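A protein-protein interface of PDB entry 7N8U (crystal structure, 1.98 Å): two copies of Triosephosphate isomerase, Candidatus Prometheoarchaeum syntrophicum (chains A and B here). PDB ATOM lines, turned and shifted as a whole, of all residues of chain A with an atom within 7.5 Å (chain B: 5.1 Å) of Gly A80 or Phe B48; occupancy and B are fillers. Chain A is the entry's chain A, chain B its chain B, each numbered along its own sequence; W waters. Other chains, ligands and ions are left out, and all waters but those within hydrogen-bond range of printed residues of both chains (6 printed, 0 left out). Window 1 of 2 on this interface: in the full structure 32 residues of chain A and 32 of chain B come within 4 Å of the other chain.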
ATOM      1  N   SER A  47      12.723  12.467   8.241  1.00  0.00           N
ATOM      2  CA  SER A  47      14.085  11.948   8.146  1.00  0.00           C
ATOM      3  C   SER A  47      14.670  12.198   6.750  1.00  0.00           C
ATOM      4  O   SER A  47      13.947  12.383   5.769  1.00  0.00           O
ATOM      5  CB  SER A  47      14.101  10.449   8.461  1.00  0.00           C
ATOM      6  OG  SER A  47      13.720  10.213   9.801  1.00  0.00           O
ATOM      7  N   PHE A  48      16.010  12.190   6.671  1.00  0.00           N
ATOM      8  CA  PHE A  48      16.706  12.531   5.425  1.00  0.00           C
ATOM      9  C   PHE A  48      16.227  11.705   4.229  1.00  0.00           C
ATOM     10  O   PHE A  48      16.207  12.199   3.099  1.00  0.00           O
ATOM     11  CB  PHE A  48      18.217  12.319   5.567  1.00  0.00           C
ATOM     12  CG  PHE A  48      18.873  13.133   6.643  1.00  0.00           C
ATOM     13  CD1 PHE A  48      19.689  12.508   7.582  1.00  0.00           C
ATOM     14  CD2 PHE A  48      18.741  14.507   6.683  1.00  0.00           C
ATOM     15  CE1 PHE A  48      20.335  13.239   8.551  1.00  0.00           C
ATOM     16  CE2 PHE A  48      19.383  15.249   7.662  1.00  0.00           C
ATOM     17  CZ  PHE A  48      20.180  14.611   8.595  1.00  0.00           C
ATOM     18  N   ASN A  49      15.898  10.424   4.444  1.00  0.00           N
ATOM     19  CA  ASN A  49      15.560   9.554   3.312  1.00  0.00           C
ATOM     20  C   ASN A  49      14.301  10.014   2.591  1.00  0.00           C
ATOM     21  O   ASN A  49      14.142   9.747   1.395  1.00  0.00           O
ATOM     22  CB  ASN A  49      15.373   8.111   3.781  1.00  0.00           C
ATOM     23  CG  ASN A  49      14.184   7.957   4.718  1.00  0.00           C
ATOM     24  OD1 ASN A  49      14.097   8.636   5.739  1.00  0.00           O
ATOM     25  ND2 ASN A  49      13.244   7.086   4.355  1.00  0.00           N
ATOM     26  N   ALA A  50      13.407  10.714   3.294  1.00  0.00           N
ATOM     27  CA  ALA A  50      12.106  11.112   2.771  1.00  0.00           C
ATOM     28  C   ALA A  50      12.025  12.581   2.359  1.00  0.00           C
ATOM     29  O   ALA A  50      11.018  12.974   1.765  1.00  0.00           O
ATOM     30  CB  ALA A  50      11.015  10.826   3.823  1.00  0.00           C
ATOM     31  N   LEU A  51      13.052  13.398   2.637  1.00  0.00           N
ATOM     32  CA  LEU A  51      12.931  14.844   2.442  1.00  0.00           C
ATOM     33  C   LEU A  51      12.571  15.196   1.004  1.00  0.00           C
ATOM     34  O   LEU A  51      11.657  15.995   0.754  1.00  0.00           O
ATOM     35  CB  LEU A  51      14.233  15.548   2.834  1.00  0.00           C
ATOM     36  CG  LEU A  51      14.470  15.600   4.341  1.00  0.00           C
ATOM     37  CD1 LEU A  51      15.842  16.210   4.649  1.00  0.00           C
ATOM     38  CD2 LEU A  51      13.315  16.349   5.057  1.00  0.00           C
ATOM     39  N   TYR A  52      13.287  14.614   0.043  1.00  0.00           N
ATOM     40  CA  TYR A  52      13.102  14.988  -1.355  1.00  0.00           C
ATOM     41  C   TYR A  52      11.696  14.630  -1.834  1.00  0.00           C
ATOM     42  O   TYR A  52      10.999  15.460  -2.429  1.00  0.00           O
ATOM     43  CB  TYR A  52      14.185  14.308  -2.201  1.00  0.00           C
ATOM     44  CG  TYR A  52      14.159  14.638  -3.673  1.00  0.00           C
ATOM     45  CD1 TYR A  52      13.449  13.849  -4.567  1.00  0.00           C
ATOM     46  CD2 TYR A  52      14.859  15.735  -4.169  1.00  0.00           C
ATOM     47  CE1 TYR A  52      13.432  14.141  -5.912  1.00  0.00           C
ATOM     48  CE2 TYR A  52      14.854  16.036  -5.526  1.00  0.00           C
ATOM     49  CZ  TYR A  52      14.139  15.234  -6.385  1.00  0.00           C
ATOM     50  OH  TYR A  52      14.121  15.523  -7.725  1.00  0.00           O
ATOM     51  N   TYR A  71      25.380  18.869   8.298  1.00  0.00           N
ATOM     52  CA  TYR A  71      26.764  19.188   8.610  1.00  0.00           C
ATOM     53  C   TYR A  71      27.033  20.666   8.313  1.00  0.00           C
ATOM     54  O   TYR A  71      26.241  21.341   7.651  1.00  0.00           O
ATOM     55  CB  TYR A  71      27.716  18.290   7.810  1.00  0.00           C
ATOM     56  CG  TYR A  71      29.090  18.218   8.415  1.00  0.00           C
ATOM     57  CD1 TYR A  71      30.228  18.390   7.635  1.00  0.00           C
ATOM     58  CD2 TYR A  71      29.251  18.002   9.776  1.00  0.00           C
ATOM     59  CE1 TYR A  71      31.495  18.345   8.203  1.00  0.00           C
ATOM     60  CE2 TYR A  71      30.504  17.955  10.345  1.00  0.00           C
ATOM     61  CZ  TYR A  71      31.616  18.124   9.560  1.00  0.00           C
ATOM     62  OH  TYR A  71      32.864  18.068  10.145  1.00  0.00           O
ATOM     63  N   ALA A  77      34.625  14.859   2.471  1.00  0.00           N
ATOM     64  CA  ALA A  77      34.807  13.476   2.910  1.00  0.00           C
ATOM     65  C   ALA A  77      34.228  13.308   4.312  1.00  0.00           C
ATOM     66  O   ALA A  77      34.942  13.216   5.316  1.00  0.00           O
ATOM     67  CB  ALA A  77      36.284  13.103   2.869  1.00  0.00           C
ATOM     68  N   PHE A  78      32.891  13.270   4.367  1.00  0.00           N
ATOM     69  CA  PHE A  78      32.153  13.185   5.632  1.00  0.00           C
ATOM     70  C   PHE A  78      31.091  12.084   5.490  1.00  0.00           C
ATOM     71  O   PHE A  78      29.905  12.345   5.266  1.00  0.00           O
ATOM     72  CB  PHE A  78      31.564  14.565   6.010  1.00  0.00           C
ATOM     73  CG  PHE A  78      32.602  15.664   6.039  1.00  0.00           C
ATOM     74  CD1 PHE A  78      33.535  15.718   7.063  1.00  0.00           C
ATOM     75  CD2 PHE A  78      32.657  16.616   5.039  1.00  0.00           C
ATOM     76  CE1 PHE A  78      34.504  16.696   7.097  1.00  0.00           C
ATOM     77  CE2 PHE A  78      33.638  17.619   5.067  1.00  0.00           C
ATOM     78  CZ  PHE A  78      34.559  17.648   6.097  1.00  0.00           C
ATOM     79  N   THR A  79      31.542  10.835   5.584  1.00  0.00           N
ATOM     80  CA  THR A  79      30.650   9.693   5.459  1.00  0.00           C
ATOM     81  C   THR A  79      29.497   9.813   6.451  1.00  0.00           C
ATOM     82  O   THR A  79      29.703  10.107   7.633  1.00  0.00           O
ATOM     83  CB  THR A  79      31.435   8.389   5.683  1.00  0.00           C
ATOM     84  OG1 THR A  79      32.525   8.307   4.743  1.00  0.00           O
ATOM     85  CG2 THR A  79      30.548   7.191   5.496  1.00  0.00           C
ATOM     86  N   GLY A  80      28.273   9.637   5.945  1.00  0.00           N
ATOM     87  CA  GLY A  80      27.068   9.666   6.746  1.00  0.00           C
ATOM     88  C   GLY A  80      26.490  11.040   7.033  1.00  0.00           C
ATOM     89  O   GLY A  80      25.444  11.118   7.693  1.00  0.00           O
ATOM     90  N   GLU A  81      27.122  12.122   6.569  1.00  0.00           N
ATOM     91  CA  GLU A  81      26.655  13.484   6.824  1.00  0.00           C
ATOM     92  C   GLU A  81      25.850  14.027   5.646  1.00  0.00           C
ATOM     93  O   GLU A  81      26.010  13.599   4.501  1.00  0.00           O
ATOM     94  CB  GLU A  81      27.827  14.428   7.105  1.00  0.00           C
ATOM     95  CG  GLU A  81      28.550  14.152   8.407  1.00  0.00           C
ATOM     96  CD  GLU A  81      27.643  14.336   9.609  1.00  0.00           C
ATOM     97  OE1 GLU A  81      27.094  15.442   9.777  1.00  0.00           O
ATOM     98  OE2 GLU A  81      27.461  13.364  10.373  1.00  0.00           O
ATOM     99  N   ILE A  82      24.998  15.007   5.933  1.00  0.00           N
ATOM    100  CA  ILE A  82      24.095  15.579   4.939  1.00  0.00           C
ATOM    101  C   ILE A  82      24.403  17.062   4.768  1.00  0.00           C
ATOM    102  O   ILE A  82      24.450  17.814   5.753  1.00  0.00           O
ATOM    103  CB  ILE A  82      22.624  15.378   5.333  1.00  0.00           C
ATOM    104  CG1 ILE A  82      22.265  13.892   5.351  1.00  0.00           C
ATOM    105  CG2 ILE A  82      21.725  16.197   4.406  1.00  0.00           C
ATOM    106  CD1 ILE A  82      22.335  13.176   3.968  1.00  0.00           C
ATOM    107  N   SER A  86      21.941  19.752   0.185  1.00  0.00           N
ATOM    108  CA  SER A  86      20.995  18.665  -0.012  1.00  0.00           C
ATOM    109  C   SER A  86      19.648  19.000   0.616  1.00  0.00           C
ATOM    110  O   SER A  86      18.591  18.623   0.086  1.00  0.00           O
ATOM    111  CB  SER A  86      21.559  17.373   0.584  1.00  0.00           C
ATOM    112  OG  SER A  86      22.723  16.962  -0.119  1.00  0.00           O
ATOM    113  N   PRO B  46      25.312   6.397  -2.035  1.00  0.00           N
ATOM    114  CA  PRO B  46      24.957   7.822  -2.039  1.00  0.00           C
ATOM    115  C   PRO B  46      24.582   8.274  -0.640  1.00  0.00           C
ATOM    116  O   PRO B  46      24.362   7.462   0.265  1.00  0.00           O
ATOM    117  CB  PRO B  46      23.746   7.898  -2.974  1.00  0.00           C
ATOM    118  CG  PRO B  46      23.694   6.551  -3.688  1.00  0.00           C
ATOM    119  CD  PRO B  46      24.343   5.570  -2.776  1.00  0.00           C
ATOM    120  N   SER B  47      24.487   9.592  -0.478  1.00  0.00           N
ATOM    121  CA  SER B  47      24.012  10.170   0.779  1.00  0.00           C
ATOM    122  C   SER B  47      22.519   9.895   0.972  1.00  0.00           C
ATOM    123  O   SER B  47      21.784   9.654   0.010  1.00  0.00           O
ATOM    124  CB  SER B  47      24.261  11.682   0.802  1.00  0.00           C
ATOM    125  OG  SER B  47      25.645  11.989   0.707  1.00  0.00           O
ATOM    126  N   PHE B  48      22.066   9.989   2.237  1.00  0.00           N
ATOM    127  CA  PHE B  48      20.705   9.573   2.596  1.00  0.00           C
ATOM    128  C   PHE B  48      19.642  10.238   1.727  1.00  0.00           C
ATOM    129  O   PHE B  48      18.601   9.637   1.440  1.00  0.00           O
ATOM    130  CB  PHE B  48      20.391   9.908   4.064  1.00  0.00           C
ATOM    131  CG  PHE B  48      21.250   9.197   5.065  1.00  0.00           C
ATOM    132  CD1 PHE B  48      21.375   7.818   5.040  1.00  0.00           C
ATOM    133  CD2 PHE B  48      21.904   9.912   6.052  1.00  0.00           C
ATOM    134  CE1 PHE B  48      22.156   7.164   5.972  1.00  0.00           C
ATOM    135  CE2 PHE B  48      22.684   9.273   6.992  1.00  0.00           C
ATOM    136  CZ  PHE B  48      22.820   7.898   6.952  1.00  0.00           C
ATOM    137  N   ASN B  49      19.858  11.502   1.353  1.00  0.00           N
ATOM    138  CA  ASN B  49      18.824  12.241   0.640  1.00  0.00           C
ATOM    139  C   ASN B  49      18.551  11.638  -0.727  1.00  0.00           C
ATOM    140  O   ASN B  49      17.441  11.771  -1.247  1.00  0.00           O
ATOM    141  CB  ASN B  49      19.222  13.714   0.463  1.00  0.00           C
ATOM    142  CG  ASN B  49      20.461  13.896  -0.427  1.00  0.00           C
ATOM    143  OD1 ASN B  49      21.493  13.269  -0.206  1.00  0.00           O
ATOM    144  ND2 ASN B  49      20.346  14.751  -1.449  1.00  0.00           N
ATOM    145  N   ALA B  50      19.543  10.979  -1.325  1.00  0.00           N
ATOM    146  CA  ALA B  50      19.396  10.450  -2.673  1.00  0.00           C
ATOM    147  C   ALA B  50      19.060   8.968  -2.725  1.00  0.00           C
ATOM    148  O   ALA B  50      18.770   8.470  -3.816  1.00  0.00           O
ATOM    149  CB  ALA B  50      20.686  10.709  -3.486  1.00  0.00           C
ATOM    150  N   LEU B  51      19.071   8.252  -1.585  1.00  0.00           N
ATOM    151  CA  LEU B  51      19.014   6.788  -1.629  1.00  0.00           C
ATOM    152  C   LEU B  51      17.773   6.297  -2.358  1.00  0.00           C
ATOM    153  O   LEU B  51      17.852   5.428  -3.239  1.00  0.00           O
ATOM    154  CB  LEU B  51      19.046   6.202  -0.215  1.00  0.00           C
ATOM    155  CG  LEU B  51      20.396   6.282   0.492  1.00  0.00           C
ATOM    156  CD1 LEU B  51      20.285   5.764   1.921  1.00  0.00           C
ATOM    157  CD2 LEU B  51      21.452   5.496  -0.294  1.00  0.00           C
ATOM    158  N   TYR B  52      16.613   6.832  -1.986  1.00  0.00           N
ATOM    159  CA  TYR B  52      15.350   6.342  -2.526  1.00  0.00           C
ATOM    160  C   TYR B  52      15.277   6.551  -4.037  1.00  0.00           C
ATOM    161  O   TYR B  52      14.917   5.637  -4.789  1.00  0.00           O
ATOM    162  CB  TYR B  52      14.197   7.053  -1.810  1.00  0.00           C
ATOM    163  CG  TYR B  52      12.825   6.510  -2.113  1.00  0.00           C
ATOM    164  CD1 TYR B  52      12.009   7.131  -3.049  1.00  0.00           C
ATOM    165  CD2 TYR B  52      12.342   5.381  -1.461  1.00  0.00           C
ATOM    166  CE1 TYR B  52      10.749   6.646  -3.325  1.00  0.00           C
ATOM    167  CE2 TYR B  52      11.078   4.890  -1.729  1.00  0.00           C
ATOM    168  CZ  TYR B  52      10.290   5.532  -2.668  1.00  0.00           C
ATOM    169  OH  TYR B  52       9.033   5.053  -2.949  1.00  0.00           O
ATOM    170  N   GLN B  68      25.432   4.815   3.836  1.00  0.00           N
ATOM    171  CA  GLN B  68      26.713   5.202   4.417  1.00  0.00           C
ATOM    172  C   GLN B  68      26.761   5.033   5.925  1.00  0.00           C
ATOM    173  O   GLN B  68      27.843   5.161   6.509  1.00  0.00           O
ATOM    174  CB  GLN B  68      27.028   6.670   4.091  1.00  0.00           C
ATOM    175  CG  GLN B  68      27.298   6.927   2.621  1.00  0.00           C
ATOM    176  CD  GLN B  68      27.648   8.373   2.343  1.00  0.00           C
ATOM    177  OE1 GLN B  68      28.014   9.135   3.252  1.00  0.00           O
ATOM    178  NE2 GLN B  68      27.511   8.771   1.084  1.00  0.00           N
ATOM    179  N   ASN B  69      25.616   4.813   6.565  1.00  0.00           N
ATOM    180  CA  ASN B  69      25.486   4.736   8.017  1.00  0.00           C
ATOM    181  C   ASN B  69      24.025   4.414   8.293  1.00  0.00           C
ATOM    182  O   ASN B  69      23.187   4.443   7.385  1.00  0.00           O
ATOM    183  CB  ASN B  69      25.891   6.051   8.710  1.00  0.00           C
ATOM    184  CG  ASN B  69      26.259   5.866  10.171  1.00  0.00           C
ATOM    185  OD1 ASN B  69      26.433   4.741  10.644  1.00  0.00           O
ATOM    186  ND2 ASN B  69      26.397   6.981  10.897  1.00  0.00           N
ATOM    187  N   MET B  70      23.732   4.126   9.556  1.00  0.00           N
ATOM    188  CA  MET B  70      22.373   3.953  10.070  1.00  0.00           C
ATOM    189  C   MET B  70      22.462   3.908  11.590  1.00  0.00           C
ATOM    190  O   MET B  70      23.553   3.832  12.154  1.00  0.00           O
ATOM    191  CB  MET B  70      21.719   2.675   9.531  1.00  0.00           C
ATOM    192  CG  MET B  70      22.356   1.407  10.091  1.00  0.00           C
ATOM    193  SD  MET B  70      21.664  -0.135   9.416  1.00  0.00           S
ATOM    194  CE  MET B  70      21.815  -1.197  10.860  1.00  0.00           C
ATOM    195  N   ILE B  82      18.987   7.667  10.939  1.00  0.00           N
ATOM    196  CA  ILE B  82      18.335   6.950   9.849  1.00  0.00           C
ATOM    197  C   ILE B  82      18.199   5.480  10.237  1.00  0.00           C
ATOM    198  O   ILE B  82      19.181   4.842  10.637  1.00  0.00           O
ATOM    199  CB  ILE B  82      19.119   7.096   8.531  1.00  0.00           C
ATOM    200  CG1 ILE B  82      19.139   8.568   8.065  1.00  0.00           C
ATOM    201  CG2 ILE B  82      18.538   6.193   7.469  1.00  0.00           C
ATOM    202  CD1 ILE B  82      17.736   9.159   7.744  1.00  0.00           C
ATOM    203  N   LEU B  87      16.774   2.332   5.069  1.00  0.00           N
ATOM    204  CA  LEU B  87      17.703   1.840   4.055  1.00  0.00           C
ATOM    205  C   LEU B  87      17.044   0.760   3.210  1.00  0.00           C
ATOM    206  O   LEU B  87      17.139   0.774   1.975  1.00  0.00           O
ATOM    207  CB  LEU B  87      18.976   1.311   4.711  1.00  0.00           C
ATOM    208  CG  LEU B  87      19.798   2.314   5.532  1.00  0.00           C
ATOM    209  CD1 LEU B  87      21.125   1.673   5.888  1.00  0.00           C
ATOM    210  CD2 LEU B  87      20.006   3.622   4.760  1.00  0.00           C
ATOM    211  N   ARG B 102      33.207   8.290  10.761  1.00  0.00           N
ATOM    212  CA  ARG B 102      32.261   8.120  11.866  1.00  0.00           C
ATOM    213  C   ARG B 102      32.992   7.888  13.182  1.00  0.00           C
ATOM    214  O   ARG B 102      32.617   8.445  14.211  1.00  0.00           O
ATOM    215  CB  ARG B 102      31.297   6.949  11.610  1.00  0.00           C
ATOM    216  CG  ARG B 102      30.485   6.976  10.328  1.00  0.00           C
ATOM    217  CD  ARG B 102      29.715   8.266  10.108  1.00  0.00           C
ATOM    218  NE  ARG B 102      29.031   8.812  11.287  1.00  0.00           N
ATOM    219  CZ  ARG B 102      28.440  10.005  11.296  1.00  0.00           C
ATOM    220  NH1 ARG B 102      28.479  10.753  10.199  1.00  0.00           N
ATOM    221  NH2 ARG B 102      27.845  10.470  12.398  1.00  0.00           N
HETATM  222  O   HOH W   1      18.064  16.468  -1.641  1.00  0.00           O
HETATM  223  O   HOH W   2      16.413   8.724   0.200  1.00  0.00           O
HETATM  224  O   HOH W   3      26.260  11.274   3.267  1.00  0.00           O
HETATM  225  O   HOH W   4      26.359  12.921  12.633  1.00  0.00           O
HETATM  226  O   HOH W   5      25.146   9.328   9.808  1.00  0.00           O
HETATM  227  O   HOH W   6      15.541  12.856   0.528  1.00  0.00           O
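The guanidinium group (NE) of Arg B102 lies close to the side-chain amide nitrogen (ND2) of Asn B69, at 3.2 Å.
The backbone NH (N) of Tyr A71 sits at hydrogen-bond distance from the backbone carbonyl oxygen (O) of Ile A82 (2.9 Å).
Ala A50 touches none of the printed residues of chain B.
Of chain B, only Phe B48, Gln B68 and Arg B102 come within 4 Å of Gly A80.
Of the printed residues of chain B, Glu A81 touches Arg B102.
Of the printed residues of chain B, Ile A82 touches Ser B47 (3.996 Å), Phe B48 (3.6 Å) and Asn B49 (3.97 Å).
Printed residues of chain A within 4 Å of Ser B47: Ile A82 (3.996 Å).
Phe B48 touches four residues of chain A.
Printed residues of chain A within 4 Å of Asn B49: Phe A48, Ile A82 and Ser A86.
Of the printed residues of chain A, Ile B82 touches Ser A47 (3.9 Å), Phe A48 (3.6 Å) and Asn A49 (3.98 Å).
The nearest residue of chain B that does not touch Gly A80 is Asn B69 (4.3 Å).
The nearest residue of chain A that does not touch Phe B48 is Glu A81 (5.3 Å).
The nearest printed residue of chain B that does not touch Ser A47 is Phe B48 (6.7 Å).
Ser A47 touches Ile B82 (CB to CD1, 3.9 Å).
CB of Phe A48 touches CB of Phe B48, at 3.6 Å.
Ile B82 touches Phe A48.
CA of Asn A49 touches O of Phe B48, at 3.6 Å.
Asn A49 touches Ile B82 (N to CD1, 3.98 Å).
Thr A79 touches Gln B68 (CA to OE1, 3.5 Å).
Gly A80 touches Phe B48 (O to CE2, 3.4 Å).
Ile A82 touches Ser B47.
CD1 of Ile A82 touches N of Phe B48 (3.6 Å).
Ile A82 touches Asn B49.
Of the 13 printed residues of chain B, 6 touch a printed residue of chain A.
Hydrophobic or aromatic side chains of chain B that line the printed part of chain A: Phe B48 and Ile B82.
Of the 14 printed residues of chain A, 8 touch a printed residue of chain B.
Printed residues of chain A that touch a printed residue of chain B: Ser A47, Phe A48, Asn A49, Thr A79, Gly A80, Glu A81, Ile A82 and Ser A86.
Hydrophobic or aromatic side chains of chain A within 4 Å of the printed part of chain B: Phe A48 and Ile A82.
Among the printed residues, 16 pairs touch across the chains.
Among the printed residues, Asp or Glu carboxylates within 4 Å of a Lys or Arg side-chain nitrogen of the other chain: Glu A81 with Arg B102 (2.8 Å).
Water W4 lies within hydrogen-bond range of OE2 of Glu A81 (2.6 Å) and NH2 of Arg B102 (2.9 Å).
Water W3 lies within hydrogen-bond range of the backbone carbonyl oxygen of Glu A81 (2.6 Å), the side-chain hydroxyl of Ser B47 (2.7 Å) and the side-chain amide oxygen of Gln B68 (2.8 Å).
Water W2 lies within hydrogen-bond range of O of Phe B48 (2.7 Å), O of Asn A49 (2.8 Å), N of Tyr B52 (2.9 Å) and N of Leu B51 (3.2 Å).
Water W6 lies within hydrogen-bond range of the backbone carbonyl oxygen (O) of Phe A48 (2.7 Å), the backbone carbonyl oxygen (O) of Asn B49 (2.8 Å), the backbone NH (N) of Tyr A52 (2.9 Å) and the backbone NH (N) of Leu A51 (3.3 Å).
Water W5 lies within hydrogen-bond range of O of Gly A80 (2.8 Å) and ND2 of Asn B69 (2.9 Å).
Water W1 lies within hydrogen-bond range of O of Ser A86 (2.8 Å) and ND2 of Asn B49 (2.9 Å).
The side-chain amide oxygen (OE1) of Gln B68 lies within hydrogen-bond range of the backbone NH (N) of Gly A80, at 2.8 Å.
NH1 of Arg B102 is in hydrogen-bond range of O of Thr A79 (2.9 Å).
The side-chain carboxylate (OE2) of Glu A81 is in salt-bridge range of the guanidinium group (NH1) of Arg B102, at 2.8 Å.
Ser A47 touches Ile B82, and with the chains exchanged Ile A82 touches Ser B47.
Phe B48 touches its own counterpart, Phe A48.
Phe A48 touches Asn B49, and with the chains exchanged Asn A49 touches Phe B48.
Asn A49 touches Ile B82, and with the chains exchanged Ile A82 touches Asn B49.
Of the 16 pairs that touch across the chains among the printed residues, 9 have their exchanged pair printed and touching as well.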
